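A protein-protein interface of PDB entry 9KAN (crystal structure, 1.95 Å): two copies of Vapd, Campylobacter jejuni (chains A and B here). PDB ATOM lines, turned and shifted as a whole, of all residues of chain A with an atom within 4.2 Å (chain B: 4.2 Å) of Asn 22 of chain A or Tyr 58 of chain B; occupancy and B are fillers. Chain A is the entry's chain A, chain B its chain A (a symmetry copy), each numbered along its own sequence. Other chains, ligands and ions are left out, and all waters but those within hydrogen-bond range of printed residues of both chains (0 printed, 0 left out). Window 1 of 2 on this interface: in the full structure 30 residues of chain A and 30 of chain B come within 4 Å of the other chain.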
ATOM      1  N   ALA A  20     -15.335  23.130  -6.237  1.00  0.00           N
ATOM      2  CA  ALA A  20     -16.236  22.054  -5.864  1.00  0.00           C
ATOM      3  C   ALA A  20     -15.484  21.067  -4.987  1.00  0.00           C
ATOM      4  O   ALA A  20     -14.325  20.729  -5.262  1.00  0.00           O
ATOM      5  CB  ALA A  20     -16.812  21.338  -7.096  1.00  0.00           C
ATOM      6  N   ILE A  21     -16.138  20.627  -3.921  1.00  0.00           N
ATOM      7  CA  ILE A  21     -15.604  19.604  -3.039  1.00  0.00           C
ATOM      8  C   ILE A  21     -16.559  18.423  -3.088  1.00  0.00           C
ATOM      9  O   ILE A  21     -17.772  18.586  -2.901  1.00  0.00           O
ATOM     10  CB  ILE A  21     -15.425  20.134  -1.603  1.00  0.00           C
ATOM     11  CG1 ILE A  21     -14.340  21.218  -1.564  1.00  0.00           C
ATOM     12  CG2 ILE A  21     -15.170  18.993  -0.626  1.00  0.00           C
ATOM     13  CD1 ILE A  21     -14.199  21.892  -0.178  1.00  0.00           C
ATOM     14  N   ASN A  22     -16.020  17.249  -3.392  1.00  0.00           N
ATOM     15  CA  ASN A  22     -16.808  16.033  -3.466  1.00  0.00           C
ATOM     16  C   ASN A  22     -16.039  14.930  -2.768  1.00  0.00           C
ATOM     17  O   ASN A  22     -14.813  14.841  -2.891  1.00  0.00           O
ATOM     18  CB  ASN A  22     -17.111  15.647  -4.919  1.00  0.00           C
ATOM     19  CG  ASN A  22     -17.839  16.749  -5.674  1.00  0.00           C
ATOM     20  OD1 ASN A  22     -19.070  16.816  -5.673  1.00  0.00           O
ATOM     21  ND2 ASN A  22     -17.078  17.640  -6.291  1.00  0.00           N
ATOM     22  N   PHE A  23     -16.757  14.094  -2.032  1.00  0.00           N
ATOM     23  CA  PHE A  23     -16.096  13.061  -1.265  1.00  0.00           C
ATOM     24  C   PHE A  23     -17.032  11.885  -1.065  1.00  0.00           C
ATOM     25  O   PHE A  23     -18.248  11.972  -1.254  1.00  0.00           O
ATOM     26  CB  PHE A  23     -15.606  13.594   0.087  1.00  0.00           C
ATOM     27  CG  PHE A  23     -16.702  14.168   0.968  1.00  0.00           C
ATOM     28  CD1 PHE A  23     -17.474  13.338   1.777  1.00  0.00           C
ATOM     29  CD2 PHE A  23     -16.932  15.538   1.007  1.00  0.00           C
ATOM     30  CE1 PHE A  23     -18.475  13.868   2.598  1.00  0.00           C
ATOM     31  CE2 PHE A  23     -17.932  16.077   1.820  1.00  0.00           C
ATOM     32  CZ  PHE A  23     -18.695  15.246   2.623  1.00  0.00           C
ATOM     33  N   SER A  59     -25.034  16.532  -5.204  1.00  0.00           N
ATOM     34  CA  SER A  59     -23.988  16.034  -4.269  1.00  0.00           C
ATOM     35  C   SER A  59     -22.771  16.967  -4.297  1.00  0.00           C
ATOM     36  O   SER A  59     -22.399  17.411  -5.406  1.00  0.00           O
ATOM     37  CB  SER A  59     -23.566  14.626  -4.608  1.00  0.00           C
ATOM     38  OG  SER A  59     -24.642  13.719  -4.421  1.00  0.00           O
ATOM     39  N   GLY A  60     -22.181  17.258  -3.133  1.00  0.00           N
ATOM     40  CA  GLY A  60     -20.934  18.049  -3.121  1.00  0.00           C
ATOM     41  C   GLY A  60     -21.085  19.446  -2.554  1.00  0.00           C
ATOM     42  O   GLY A  60     -22.236  19.878  -2.330  1.00  0.00           O
ATOM     43  N   PHE A  93     -11.813  12.061  -1.930  1.00  0.00           N
ATOM     44  CA  PHE A  93     -12.005  13.460  -1.544  1.00  0.00           C
ATOM     45  C   PHE A  93     -11.300  14.317  -2.587  1.00  0.00           C
ATOM     46  O   PHE A  93     -10.062  14.316  -2.653  1.00  0.00           O
ATOM     47  CB  PHE A  93     -11.453  13.709  -0.134  1.00  0.00           C
ATOM     48  CG  PHE A  93     -11.966  14.957   0.531  1.00  0.00           C
ATOM     49  CD1 PHE A  93     -11.583  16.209   0.090  1.00  0.00           C
ATOM     50  CD2 PHE A  93     -12.803  14.872   1.641  1.00  0.00           C
ATOM     51  CE1 PHE A  93     -12.034  17.367   0.731  1.00  0.00           C
ATOM     52  CE2 PHE A  93     -13.267  16.022   2.288  1.00  0.00           C
ATOM     53  CZ  PHE A  93     -12.883  17.270   1.829  1.00  0.00           C
ATOM     54  N   ASP A  94     -12.079  15.038  -3.394  1.00  0.00           N
ATOM     55  CA  ASP A  94     -11.560  15.775  -4.540  1.00  0.00           C
ATOM     56  C   ASP A  94     -11.928  17.251  -4.446  1.00  0.00           C
ATOM     57  O   ASP A  94     -13.035  17.596  -4.028  1.00  0.00           O
ATOM     58  CB  ASP A  94     -12.096  15.190  -5.863  1.00  0.00           C
ATOM     59  CG  ASP A  94     -11.647  13.748  -6.092  1.00  0.00           C
ATOM     60  OD1 ASP A  94     -10.506  13.399  -5.728  1.00  0.00           O
ATOM     61  OD2 ASP A  94     -12.440  12.948  -6.624  1.00  0.00           O
ATOM     62  N   ARG B  56     -19.195   9.002 -10.959  1.00  0.00           N
ATOM     63  CA  ARG B  56     -18.238   9.281  -9.861  1.00  0.00           C
ATOM     64  C   ARG B  56     -18.623   8.442  -8.640  1.00  0.00           C
ATOM     65  O   ARG B  56     -19.804   8.039  -8.544  1.00  0.00           O
ATOM     66  CB  ARG B  56     -18.277  10.771  -9.511  1.00  0.00           C
ATOM     67  CG  ARG B  56     -17.967  11.696 -10.679  1.00  0.00           C
ATOM     68  CD  ARG B  56     -16.807  11.185 -11.516  1.00  0.00           C
ATOM     69  NE  ARG B  56     -15.511  11.636 -10.999  1.00  0.00           N
ATOM     70  CZ  ARG B  56     -14.527  10.826 -10.633  1.00  0.00           C
ATOM     71  NH1 ARG B  56     -14.773   9.807  -9.830  1.00  0.00           N
ATOM     72  NH2 ARG B  56     -13.300  11.040 -11.071  1.00  0.00           N
ATOM     73  N   GLN B  57     -17.670   8.213  -7.736  1.00  0.00           N
ATOM     74  CA  GLN B  57     -17.960   7.458  -6.490  1.00  0.00           C
ATOM     75  C   GLN B  57     -18.609   8.412  -5.477  1.00  0.00           C
ATOM     76  O   GLN B  57     -18.711   8.035  -4.289  1.00  0.00           O
ATOM     77  CB  GLN B  57     -16.662   6.866  -5.943  1.00  0.00           C
ATOM     78  CG  GLN B  57     -15.605   7.908  -5.590  1.00  0.00           C
ATOM     79  CD  GLN B  57     -14.696   8.266  -6.745  1.00  0.00           C
ATOM     80  OE1 GLN B  57     -14.895   7.831  -7.885  1.00  0.00           O
ATOM     81  NE2 GLN B  57     -13.685   9.073  -6.462  1.00  0.00           N
ATOM     82  N   TYR B  58     -19.010   9.594  -5.944  1.00  0.00           N
ATOM     83  CA  TYR B  58     -19.723  10.559  -5.066  1.00  0.00           C
ATOM     84  C   TYR B  58     -21.066  10.833  -5.734  1.00  0.00           C
ATOM     85  O   TYR B  58     -22.091  10.360  -5.192  1.00  0.00           O
ATOM     86  CB  TYR B  58     -18.897  11.828  -4.819  1.00  0.00           C
ATOM     87  CG  TYR B  58     -18.568  12.695  -6.028  1.00  0.00           C
ATOM     88  CD1 TYR B  58     -19.421  13.712  -6.444  1.00  0.00           C
ATOM     89  CD2 TYR B  58     -17.422  12.469  -6.777  1.00  0.00           C
ATOM     90  CE1 TYR B  58     -19.128  14.494  -7.548  1.00  0.00           C
ATOM     91  CE2 TYR B  58     -17.120  13.238  -7.887  1.00  0.00           C
ATOM     92  CZ  TYR B  58     -17.975  14.254  -8.274  1.00  0.00           C
ATOM     93  OH  TYR B  58     -17.677  15.015  -9.366  1.00  0.00           O
ATOM     94  N   SER B  59     -21.053  11.513  -6.886  1.00  0.00           N
ATOM     95  CA  SER B  59     -22.301  11.792  -7.648  1.00  0.00           C
ATOM     96  C   SER B  59     -21.969  12.534  -8.948  1.00  0.00           C
ATOM     97  O   SER B  59     -21.099  13.432  -8.905  1.00  0.00           O
ATOM     98  CB  SER B  59     -23.281  12.598  -6.831  1.00  0.00           C
ATOM     99  OG  SER B  59     -23.732  11.855  -5.708  1.00  0.00           O
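The side-chain hydroxyl (OG) of Ser 59 of chain B lies within hydrogen-bond range of the side-chain hydroxyl (OG) of Ser 59 of chain A (2.4 Å).
OD1 of Asn 22 of chain A sits close to O of Ser 59 of chain A (3.4 Å). The backbone NH (N) of Asp 94 of chain A lies within hydrogen-bond range of the backbone carbonyl oxygen (O) of Asn 22 of chain A, at 2.8 Å.
Asn 22 of chain A touches Tyr 58 of chain B (OD1 to CE1, 3.0 Å). O of Phe 23 of chain A touches CB of Tyr 58 of chain B (3.6 Å).
Asn 22 of chain A touches just one residue of chain B: Tyr 58. Tyr 58 of chain B touches two residues of chain A. Printed residues of chain A within 4 Å of Ser 59 of chain B: Ser 59 (2.4 Å). Of the printed residues of chain B, Phe 23 of chain A touches Tyr 58. Of the printed residues of chain B, Ser 59 of chain A touches Ser 59. Ile 21 of chain A touches none of the printed residues of chain B. Arg 56 of chain B touches none of the printed residues of chain A.
Of the 8 printed residues of chain A, 3 touch a printed residue of chain B. Along chain B the printed residues that touch a printed residue of chain A span positions 58 to 59. Among the printed residues, no Asp or Glu carboxylate lies within 4 Å of a Lys or Arg side-chain nitrogen of the other chain.
Ser 59 of chain B touches its own counterpart, Ser 59 of chain A. Position printed for both chains: 59. Of the 3 pairs that touch across the chains among the printed residues, 1 has its exchanged pair printed and touching as well.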
